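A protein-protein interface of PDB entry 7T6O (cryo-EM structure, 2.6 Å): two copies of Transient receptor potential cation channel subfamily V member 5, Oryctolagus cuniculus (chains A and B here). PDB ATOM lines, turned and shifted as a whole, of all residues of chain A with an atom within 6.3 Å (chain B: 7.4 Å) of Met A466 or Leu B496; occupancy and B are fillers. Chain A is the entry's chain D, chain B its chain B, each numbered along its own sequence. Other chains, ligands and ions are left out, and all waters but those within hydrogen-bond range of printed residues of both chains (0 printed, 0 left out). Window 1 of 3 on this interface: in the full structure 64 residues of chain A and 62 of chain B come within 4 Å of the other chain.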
ATOM      1  N   PHE A 425     -37.564  18.966 -10.739  1.00  0.00           N
ATOM      2  CA  PHE A 425     -36.444  18.692 -11.630  1.00  0.00           C
ATOM      3  C   PHE A 425     -36.807  18.955 -13.084  1.00  0.00           C
ATOM      4  O   PHE A 425     -35.970  19.455 -13.844  1.00  0.00           O
ATOM      5  CB  PHE A 425     -35.958  17.258 -11.436  1.00  0.00           C
ATOM      6  CG  PHE A 425     -35.172  17.060 -10.176  1.00  0.00           C
ATOM      7  CD1 PHE A 425     -33.931  17.661 -10.021  1.00  0.00           C
ATOM      8  CD2 PHE A 425     -35.677  16.291  -9.141  1.00  0.00           C
ATOM      9  CE1 PHE A 425     -33.205  17.490  -8.859  1.00  0.00           C
ATOM     10  CE2 PHE A 425     -34.954  16.114  -7.976  1.00  0.00           C
ATOM     11  CZ  PHE A 425     -33.717  16.713  -7.836  1.00  0.00           C
ATOM     12  N   TRP A 462     -26.453  22.009 -13.107  1.00  0.00           N
ATOM     13  CA  TRP A 462     -25.745  21.111 -12.208  1.00  0.00           C
ATOM     14  C   TRP A 462     -26.665  20.568 -11.127  1.00  0.00           C
ATOM     15  O   TRP A 462     -26.577  19.386 -10.802  1.00  0.00           O
ATOM     16  CB  TRP A 462     -24.529  21.798 -11.599  1.00  0.00           C
ATOM     17  CG  TRP A 462     -23.288  21.661 -12.439  1.00  0.00           C
ATOM     18  CD1 TRP A 462     -22.631  22.658 -13.097  1.00  0.00           C
ATOM     19  CD2 TRP A 462     -22.561  20.455 -12.714  1.00  0.00           C
ATOM     20  NE1 TRP A 462     -21.542  22.154 -13.760  1.00  0.00           N
ATOM     21  CE2 TRP A 462     -21.476  20.803 -13.543  1.00  0.00           C
ATOM     22  CE3 TRP A 462     -22.720  19.117 -12.338  1.00  0.00           C
ATOM     23  CZ2 TRP A 462     -20.556  19.863 -14.003  1.00  0.00           C
ATOM     24  CZ3 TRP A 462     -21.807  18.185 -12.799  1.00  0.00           C
ATOM     25  CH2 TRP A 462     -20.739  18.562 -13.621  1.00  0.00           C
ATOM     26  N   CYS A 463     -27.599  21.375 -10.610  1.00  0.00           N
ATOM     27  CA  CYS A 463     -28.571  20.861  -9.649  1.00  0.00           C
ATOM     28  C   CYS A 463     -29.543  19.857 -10.266  1.00  0.00           C
ATOM     29  O   CYS A 463     -30.182  19.101  -9.530  1.00  0.00           O
ATOM     30  CB  CYS A 463     -29.349  22.017  -9.020  1.00  0.00           C
ATOM     31  SG  CYS A 463     -28.452  22.892  -7.715  1.00  0.00           S
ATOM     32  N   SER A 464     -29.664  19.834 -11.596  1.00  0.00           N
ATOM     33  CA  SER A 464     -30.473  18.825 -12.268  1.00  0.00           C
ATOM     34  C   SER A 464     -29.817  17.445 -12.295  1.00  0.00           C
ATOM     35  O   SER A 464     -30.482  16.472 -12.664  1.00  0.00           O
ATOM     36  CB  SER A 464     -30.781  19.271 -13.696  1.00  0.00           C
ATOM     37  OG  SER A 464     -31.503  20.487 -13.709  1.00  0.00           O
ATOM     38  N   VAL A 465     -28.534  17.335 -11.930  1.00  0.00           N
ATOM     39  CA  VAL A 465     -27.891  16.031 -11.765  1.00  0.00           C
ATOM     40  C   VAL A 465     -28.500  15.277 -10.585  1.00  0.00           C
ATOM     41  O   VAL A 465     -28.553  14.041 -10.590  1.00  0.00           O
ATOM     42  CB  VAL A 465     -26.355  16.219 -11.629  1.00  0.00           C
ATOM     43  CG1 VAL A 465     -25.611  14.899 -11.462  1.00  0.00           C
ATOM     44  CG2 VAL A 465     -25.808  16.945 -12.844  1.00  0.00           C
ATOM     45  N   MET A 466     -29.049  16.003  -9.606  1.00  0.00           N
ATOM     46  CA  MET A 466     -29.726  15.412  -8.456  1.00  0.00           C
ATOM     47  C   MET A 466     -31.021  14.689  -8.817  1.00  0.00           C
ATOM     48  O   MET A 466     -31.582  14.009  -7.952  1.00  0.00           O
ATOM     49  CB  MET A 466     -30.016  16.498  -7.418  1.00  0.00           C
ATOM     50  CG  MET A 466     -28.892  16.722  -6.425  1.00  0.00           C
ATOM     51  SD  MET A 466     -29.369  17.736  -5.016  1.00  0.00           S
ATOM     52  CE  MET A 466     -29.044  19.374  -5.654  1.00  0.00           C
ATOM     53  N   TYR A 467     -31.523  14.845 -10.048  1.00  0.00           N
ATOM     54  CA  TYR A 467     -32.611  14.000 -10.532  1.00  0.00           C
ATOM     55  C   TYR A 467     -32.188  12.539 -10.597  1.00  0.00           C
ATOM     56  O   TYR A 467     -32.976  11.640 -10.283  1.00  0.00           O
ATOM     57  CB  TYR A 467     -33.076  14.481 -11.908  1.00  0.00           C
ATOM     58  CG  TYR A 467     -34.075  13.559 -12.580  1.00  0.00           C
ATOM     59  CD1 TYR A 467     -35.412  13.572 -12.206  1.00  0.00           C
ATOM     60  CD2 TYR A 467     -33.684  12.691 -13.597  1.00  0.00           C
ATOM     61  CE1 TYR A 467     -36.329  12.736 -12.809  1.00  0.00           C
ATOM     62  CE2 TYR A 467     -34.594  11.849 -14.204  1.00  0.00           C
ATOM     63  CZ  TYR A 467     -35.916  11.879 -13.806  1.00  0.00           C
ATOM     64  OH  TYR A 467     -36.832  11.051 -14.407  1.00  0.00           O
ATOM     65  N   PHE A 468     -30.944  12.280 -11.000  1.00  0.00           N
ATOM     66  CA  PHE A 468     -30.438  10.924 -11.164  1.00  0.00           C
ATOM     67  C   PHE A 468     -30.052  10.262  -9.850  1.00  0.00           C
ATOM     68  O   PHE A 468     -29.546   9.136  -9.866  1.00  0.00           O
ATOM     69  CB  PHE A 468     -29.245  10.921 -12.117  1.00  0.00           C
ATOM     70  CG  PHE A 468     -29.594  11.330 -13.514  1.00  0.00           C
ATOM     71  CD1 PHE A 468     -30.193  10.429 -14.382  1.00  0.00           C
ATOM     72  CD2 PHE A 468     -29.331  12.615 -13.961  1.00  0.00           C
ATOM     73  CE1 PHE A 468     -30.518  10.800 -15.669  1.00  0.00           C
ATOM     74  CE2 PHE A 468     -29.655  12.992 -15.248  1.00  0.00           C
ATOM     75  CZ  PHE A 468     -30.249  12.083 -16.103  1.00  0.00           C
ATOM     76  N   ALA A 469     -30.284  10.928  -8.718  1.00  0.00           N
ATOM     77  CA  ALA A 469     -30.143  10.327  -7.401  1.00  0.00           C
ATOM     78  C   ALA A 469     -31.208   9.277  -7.111  1.00  0.00           C
ATOM     79  O   ALA A 469     -31.045   8.511  -6.157  1.00  0.00           O
ATOM     80  CB  ALA A 469     -30.194  11.423  -6.341  1.00  0.00           C
ATOM     81  N   ARG A 470     -32.272   9.218  -7.922  1.00  0.00           N
ATOM     82  CA  ARG A 470     -33.360   8.261  -7.731  1.00  0.00           C
ATOM     83  C   ARG A 470     -32.896   6.819  -7.900  1.00  0.00           C
ATOM     84  O   ARG A 470     -33.517   5.895  -7.364  1.00  0.00           O
ATOM     85  CB  ARG A 470     -34.478   8.562  -8.728  1.00  0.00           C
ATOM     86  CG  ARG A 470     -35.309   9.756  -8.365  1.00  0.00           C
ATOM     87  CD  ARG A 470     -36.117  10.272  -9.547  1.00  0.00           C
ATOM     88  NE  ARG A 470     -37.086  11.277  -9.125  1.00  0.00           N
ATOM     89  CZ  ARG A 470     -36.791  12.543  -8.864  1.00  0.00           C
ATOM     90  NH1 ARG A 470     -35.559  13.008  -8.985  1.00  0.00           N
ATOM     91  NH2 ARG A 470     -37.756  13.364  -8.459  1.00  0.00           N
ATOM     92  N   LEU A 475     -28.765   8.025  -2.160  1.00  0.00           N
ATOM     93  CA  LEU A 475     -28.916   9.420  -2.553  1.00  0.00           C
ATOM     94  C   LEU A 475     -30.367   9.868  -2.699  1.00  0.00           C
ATOM     95  O   LEU A 475     -30.678  11.024  -2.379  1.00  0.00           O
ATOM     96  CB  LEU A 475     -28.180   9.648  -3.876  1.00  0.00           C
ATOM     97  CG  LEU A 475     -26.701   9.270  -3.939  1.00  0.00           C
ATOM     98  CD1 LEU A 475     -26.170   9.419  -5.356  1.00  0.00           C
ATOM     99  CD2 LEU A 475     -25.893  10.105  -2.978  1.00  0.00           C
ATOM    100  N   PHE A 478     -32.368  11.063   0.463  1.00  0.00           N
ATOM    101  CA  PHE A 478     -31.850  12.348   0.919  1.00  0.00           C
ATOM    102  C   PHE A 478     -32.260  13.478  -0.020  1.00  0.00           C
ATOM    103  O   PHE A 478     -32.509  14.600   0.429  1.00  0.00           O
ATOM    104  CB  PHE A 478     -30.330  12.290   1.066  1.00  0.00           C
ATOM    105  CG  PHE A 478     -29.755  13.458   1.815  1.00  0.00           C
ATOM    106  CD1 PHE A 478     -29.933  13.573   3.186  1.00  0.00           C
ATOM    107  CD2 PHE A 478     -29.043  14.443   1.153  1.00  0.00           C
ATOM    108  CE1 PHE A 478     -29.410  14.651   3.879  1.00  0.00           C
ATOM    109  CE2 PHE A 478     -28.515  15.522   1.841  1.00  0.00           C
ATOM    110  CZ  PHE A 478     -28.700  15.625   3.205  1.00  0.00           C
ATOM    111  N   THR A 479     -32.353  13.197  -1.323  1.00  0.00           N
ATOM    112  CA  THR A 479     -32.823  14.212  -2.265  1.00  0.00           C
ATOM    113  C   THR A 479     -34.306  14.513  -2.063  1.00  0.00           C
ATOM    114  O   THR A 479     -34.740  15.668  -2.196  1.00  0.00           O
ATOM    115  CB  THR A 479     -32.547  13.755  -3.697  1.00  0.00           C
ATOM    116  OG1 THR A 479     -31.218  13.231  -3.772  1.00  0.00           O
ATOM    117  CG2 THR A 479     -32.667  14.918  -4.668  1.00  0.00           C
ATOM    118  N   ILE A 482     -34.385  16.762   0.836  1.00  0.00           N
ATOM    119  CA  ILE A 482     -34.013  18.115   0.418  1.00  0.00           C
ATOM    120  C   ILE A 482     -35.207  18.836  -0.202  1.00  0.00           C
ATOM    121  O   ILE A 482     -35.489  19.998   0.122  1.00  0.00           O
ATOM    122  CB  ILE A 482     -32.818  18.064  -0.555  1.00  0.00           C
ATOM    123  CG1 ILE A 482     -31.529  17.712   0.184  1.00  0.00           C
ATOM    124  CG2 ILE A 482     -32.631  19.384  -1.293  1.00  0.00           C
ATOM    125  CD1 ILE A 482     -30.414  17.283  -0.740  1.00  0.00           C
ATOM    126  N   MET B 491     -20.430   9.680   2.822  1.00  0.00           N
ATOM    127  CA  MET B 491     -20.213   9.320   1.425  1.00  0.00           C
ATOM    128  C   MET B 491     -21.387   9.738   0.551  1.00  0.00           C
ATOM    129  O   MET B 491     -21.186  10.305  -0.526  1.00  0.00           O
ATOM    130  CB  MET B 491     -19.962   7.817   1.306  1.00  0.00           C
ATOM    131  CG  MET B 491     -19.249   7.412   0.029  1.00  0.00           C
ATOM    132  SD  MET B 491     -17.468   7.674   0.121  1.00  0.00           S
ATOM    133  CE  MET B 491     -17.249   8.952  -1.115  1.00  0.00           C
ATOM    134  N   ARG B 492     -22.622   9.511   1.016  1.00  0.00           N
ATOM    135  CA  ARG B 492     -23.789   9.921   0.238  1.00  0.00           C
ATOM    136  C   ARG B 492     -23.971  11.434   0.263  1.00  0.00           C
ATOM    137  O   ARG B 492     -24.602  12.005  -0.633  1.00  0.00           O
ATOM    138  CB  ARG B 492     -25.053   9.212   0.743  1.00  0.00           C
ATOM    139  CG  ARG B 492     -25.795   9.904   1.883  1.00  0.00           C
ATOM    140  CD  ARG B 492     -26.937   9.057   2.416  1.00  0.00           C
ATOM    141  NE  ARG B 492     -26.467   7.862   3.107  1.00  0.00           N
ATOM    142  CZ  ARG B 492     -27.256   6.902   3.566  1.00  0.00           C
ATOM    143  NH1 ARG B 492     -28.570   6.960   3.426  1.00  0.00           N
ATOM    144  NH2 ARG B 492     -26.713   5.857   4.183  1.00  0.00           N
ATOM    145  N   PHE B 493     -23.421  12.106   1.273  1.00  0.00           N
ATOM    146  CA  PHE B 493     -23.483  13.558   1.299  1.00  0.00           C
ATOM    147  C   PHE B 493     -22.482  14.152   0.320  1.00  0.00           C
ATOM    148  O   PHE B 493     -22.703  15.244  -0.218  1.00  0.00           O
ATOM    149  CB  PHE B 493     -23.217  14.061   2.714  1.00  0.00           C
ATOM    150  CG  PHE B 493     -23.487  15.522   2.901  1.00  0.00           C
ATOM    151  CD1 PHE B 493     -24.683  16.076   2.475  1.00  0.00           C
ATOM    152  CD2 PHE B 493     -22.554  16.339   3.520  1.00  0.00           C
ATOM    153  CE1 PHE B 493     -24.943  17.420   2.653  1.00  0.00           C
ATOM    154  CE2 PHE B 493     -22.808  17.685   3.701  1.00  0.00           C
ATOM    155  CZ  PHE B 493     -24.006  18.223   3.269  1.00  0.00           C
ATOM    156  N   CYS B 494     -21.380  13.434   0.077  1.00  0.00           N
ATOM    157  CA  CYS B 494     -20.298  13.954  -0.753  1.00  0.00           C
ATOM    158  C   CYS B 494     -20.692  14.118  -2.219  1.00  0.00           C
ATOM    159  O   CYS B 494     -20.212  15.050  -2.869  1.00  0.00           O
ATOM    160  CB  CYS B 494     -19.067  13.056  -0.635  1.00  0.00           C
ATOM    161  SG  CYS B 494     -18.021  13.419   0.796  1.00  0.00           S
ATOM    162  N   TRP B 495     -21.554  13.244  -2.760  1.00  0.00           N
ATOM    163  CA  TRP B 495     -21.954  13.386  -4.163  1.00  0.00           C
ATOM    164  C   TRP B 495     -22.777  14.648  -4.391  1.00  0.00           C
ATOM    165  O   TRP B 495     -22.470  15.444  -5.284  1.00  0.00           O
ATOM    166  CB  TRP B 495     -22.740  12.168  -4.659  1.00  0.00           C
ATOM    167  CG  TRP B 495     -22.107  10.843  -4.434  1.00  0.00           C
ATOM    168  CD1 TRP B 495     -22.239  10.050  -3.344  1.00  0.00           C
ATOM    169  CD2 TRP B 495     -21.228  10.155  -5.330  1.00  0.00           C
ATOM    170  NE1 TRP B 495     -21.501   8.902  -3.496  1.00  0.00           N
ATOM    171  CE2 TRP B 495     -20.869   8.943  -4.711  1.00  0.00           C
ATOM    172  CE3 TRP B 495     -20.711  10.446  -6.596  1.00  0.00           C
ATOM    173  CZ2 TRP B 495     -20.016   8.021  -5.312  1.00  0.00           C
ATOM    174  CZ3 TRP B 495     -19.865   9.529  -7.192  1.00  0.00           C
ATOM    175  CH2 TRP B 495     -19.526   8.332  -6.550  1.00  0.00           C
ATOM    176  N   LEU B 496     -23.816  14.856  -3.579  1.00  0.00           N
ATOM    177  CA  LEU B 496     -24.653  16.041  -3.742  1.00  0.00           C
ATOM    178  C   LEU B 496     -23.907  17.302  -3.328  1.00  0.00           C
ATOM    179  O   LEU B 496     -24.147  18.382  -3.888  1.00  0.00           O
ATOM    180  CB  LEU B 496     -25.946  15.883  -2.939  1.00  0.00           C
ATOM    181  CG  LEU B 496     -26.696  14.551  -3.075  1.00  0.00           C
ATOM    182  CD1 LEU B 496     -27.987  14.593  -2.289  1.00  0.00           C
ATOM    183  CD2 LEU B 496     -26.975  14.180  -4.524  1.00  0.00           C
ATOM    184  N   MET B 497     -22.973  17.165  -2.382  1.00  0.00           N
ATOM    185  CA  MET B 497     -22.065  18.246  -2.025  1.00  0.00           C
ATOM    186  C   MET B 497     -21.193  18.653  -3.205  1.00  0.00           C
ATOM    187  O   MET B 497     -21.032  19.847  -3.479  1.00  0.00           O
ATOM    188  CB  MET B 497     -21.221  17.773  -0.842  1.00  0.00           C
ATOM    189  CG  MET B 497     -20.250  18.747  -0.244  1.00  0.00           C
ATOM    190  SD  MET B 497     -19.486  17.933   1.172  1.00  0.00           S
ATOM    191  CE  MET B 497     -18.302  19.160   1.696  1.00  0.00           C
ATOM    192  N   ALA B 498     -20.653  17.672  -3.937  1.00  0.00           N
ATOM    193  CA  ALA B 498     -19.834  17.959  -5.110  1.00  0.00           C
ATOM    194  C   ALA B 498     -20.666  18.555  -6.236  1.00  0.00           C
ATOM    195  O   ALA B 498     -20.184  19.408  -6.984  1.00  0.00           O
ATOM    196  CB  ALA B 498     -19.131  16.687  -5.579  1.00  0.00           C
ATOM    197  N   VAL B 499     -21.918  18.111  -6.363  1.00  0.00           N
ATOM    198  CA  VAL B 499     -22.856  18.673  -7.338  1.00  0.00           C
ATOM    199  C   VAL B 499     -23.105  20.160  -7.087  1.00  0.00           C
ATOM    200  O   VAL B 499     -22.965  20.999  -7.995  1.00  0.00           O
ATOM    201  CB  VAL B 499     -24.166  17.863  -7.310  1.00  0.00           C
ATOM    202  CG1 VAL B 499     -25.207  18.540  -8.086  1.00  0.00           C
ATOM    203  CG2 VAL B 499     -23.943  16.510  -7.956  1.00  0.00           C
ATOM    204  N   VAL B 500     -23.453  20.506  -5.842  1.00  0.00           N
ATOM    205  CA  VAL B 500     -23.734  21.896  -5.489  1.00  0.00           C
ATOM    206  C   VAL B 500     -22.469  22.746  -5.582  1.00  0.00           C
ATOM    207  O   VAL B 500     -22.504  23.886  -6.070  1.00  0.00           O
ATOM    208  CB  VAL B 500     -24.383  21.951  -4.092  1.00  0.00           C
ATOM    209  CG1 VAL B 500     -24.535  23.378  -3.595  1.00  0.00           C
ATOM    210  CG2 VAL B 500     -25.740  21.281  -4.132  1.00  0.00           C
ATOM    211  N   ILE B 501     -21.326  22.181  -5.172  1.00  0.00           N
ATOM    212  CA  ILE B 501     -20.051  22.889  -5.239  1.00  0.00           C
ATOM    213  C   ILE B 501     -19.651  23.152  -6.686  1.00  0.00           C
ATOM    214  O   ILE B 501     -19.211  24.255  -7.015  1.00  0.00           O
ATOM    215  CB  ILE B 501     -18.974  22.105  -4.460  1.00  0.00           C
ATOM    216  CG1 ILE B 501     -19.053  22.440  -2.970  1.00  0.00           C
ATOM    217  CG2 ILE B 501     -17.562  22.387  -4.970  1.00  0.00           C
ATOM    218  CD1 ILE B 501     -18.406  21.408  -2.089  1.00  0.00           C
ATOM    219  N   LEU B 502     -19.852  22.175  -7.579  1.00  0.00           N
ATOM    220  CA  LEU B 502     -19.516  22.350  -8.992  1.00  0.00           C
ATOM    221  C   LEU B 502     -20.364  23.436  -9.641  1.00  0.00           C
ATOM    222  O   LEU B 502     -19.830  24.334 -10.308  1.00  0.00           O
ATOM    223  CB  LEU B 502     -19.689  21.028  -9.742  1.00  0.00           C
ATOM    224  CG  LEU B 502     -18.498  20.072  -9.797  1.00  0.00           C
ATOM    225  CD1 LEU B 502     -18.946  18.708 -10.292  1.00  0.00           C
ATOM    226  CD2 LEU B 502     -17.401  20.632 -10.681  1.00  0.00           C
ATOM    227  N   PHE B 537     -19.059  26.286   1.557  1.00  0.00           N
ATOM    228  CA  PHE B 537     -20.077  25.282   1.841  1.00  0.00           C
ATOM    229  C   PHE B 537     -20.097  24.949   3.324  1.00  0.00           C
ATOM    230  O   PHE B 537     -21.151  24.962   3.965  1.00  0.00           O
ATOM    231  CB  PHE B 537     -19.798  24.012   1.035  1.00  0.00           C
ATOM    232  CG  PHE B 537     -20.822  22.938   1.230  1.00  0.00           C
ATOM    233  CD1 PHE B 537     -22.046  23.030   0.614  1.00  0.00           C
ATOM    234  CD2 PHE B 537     -20.588  21.871   2.083  1.00  0.00           C
ATOM    235  CE1 PHE B 537     -23.010  22.061   0.795  1.00  0.00           C
ATOM    236  CE2 PHE B 537     -21.550  20.905   2.282  1.00  0.00           C
ATOM    237  CZ  PHE B 537     -22.763  21.001   1.630  1.00  0.00           C
ATOM    238  N   ILE B 565     -29.378  27.427   0.261  1.00  0.00           N
ATOM    239  CA  ILE B 565     -29.500  26.024  -0.132  1.00  0.00           C
ATOM    240  C   ILE B 565     -28.413  25.177   0.518  1.00  0.00           C
ATOM    241  O   ILE B 565     -28.689  24.127   1.107  1.00  0.00           O
ATOM    242  CB  ILE B 565     -29.478  25.895  -1.668  1.00  0.00           C
ATOM    243  CG1 ILE B 565     -30.698  26.585  -2.286  1.00  0.00           C
ATOM    244  CG2 ILE B 565     -29.417  24.435  -2.095  1.00  0.00           C
ATOM    245  CD1 ILE B 565     -32.027  26.122  -1.717  1.00  0.00           C
ATOM    246  N   MET B 570     -28.591  22.088   3.542  1.00  0.00           N
ATOM    247  CA  MET B 570     -28.022  20.766   3.285  1.00  0.00           C
ATOM    248  C   MET B 570     -27.069  20.330   4.392  1.00  0.00           C
ATOM    249  O   MET B 570     -27.009  19.137   4.724  1.00  0.00           O
ATOM    250  CB  MET B 570     -27.316  20.746   1.932  1.00  0.00           C
ATOM    251  CG  MET B 570     -28.232  20.396   0.772  1.00  0.00           C
ATOM    252  SD  MET B 570     -27.497  20.750  -0.833  1.00  0.00           S
ATOM    253  CE  MET B 570     -26.680  19.189  -1.161  1.00  0.00           C
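Among the printed residues, merely in contact across the chains: Trp A462 with Val B499, Leu A475 with Arg B492, Phe A478 with Leu B496, Leu A475 with Trp B495, Met A466 with Leu B496, Trp A462 with Leu B502, Thr A479 with Leu B496, Phe A478 with Phe B493 and Ile A482 with Leu B496.
The backbone carbonyl oxygen (O) of Met B491 lies close to the indole nitrogen (NE1) of Trp B495 (3.3 Å). The side-chain hydroxyl of Thr A479 is in hydrogen-bond range of the backbone carbonyl oxygen of Leu A475 (2.7 Å).
Of the 15 printed residues of chain B, 6 touch a printed residue of chain A. Hydrophobic or aromatic side chains of chain B within 4 Å of the printed part of chain A: Phe B493, Trp B495, Leu B496, Val B499 and Leu B502. Of the 14 printed residues of chain A, 6 touch a printed residue of chain B. Among the printed residues, no Asp or Glu carboxylate lies within 4 Å of a Lys or Arg side-chain nitrogen of the other chain.
Met A466 touches just one residue of chain B: Leu B496. Leu B496 touches just these residues of chain A: Met A466, Phe A478, Thr A479 and Ile A482. Of the printed residues of chain B, Thr A479 touches Leu B496. Printed residues of chain A within 4 Å of Val B499: Trp A462. Printed residues of chain A within 4 Å of Phe B493: Phe A478. Ala A469 touches none of the printed residues of chain B. The nearest residue of chain A that does not touch Leu B496 is Leu A475 (4.5 Å). The nearest printed residue of chain B that does not touch Phe A478 is Met B570 (4.2 Å).
No position is printed for both chains. Of the 9 pairs that touch across the chains among the printed residues, none has its exchanged pair printed and touching as well.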
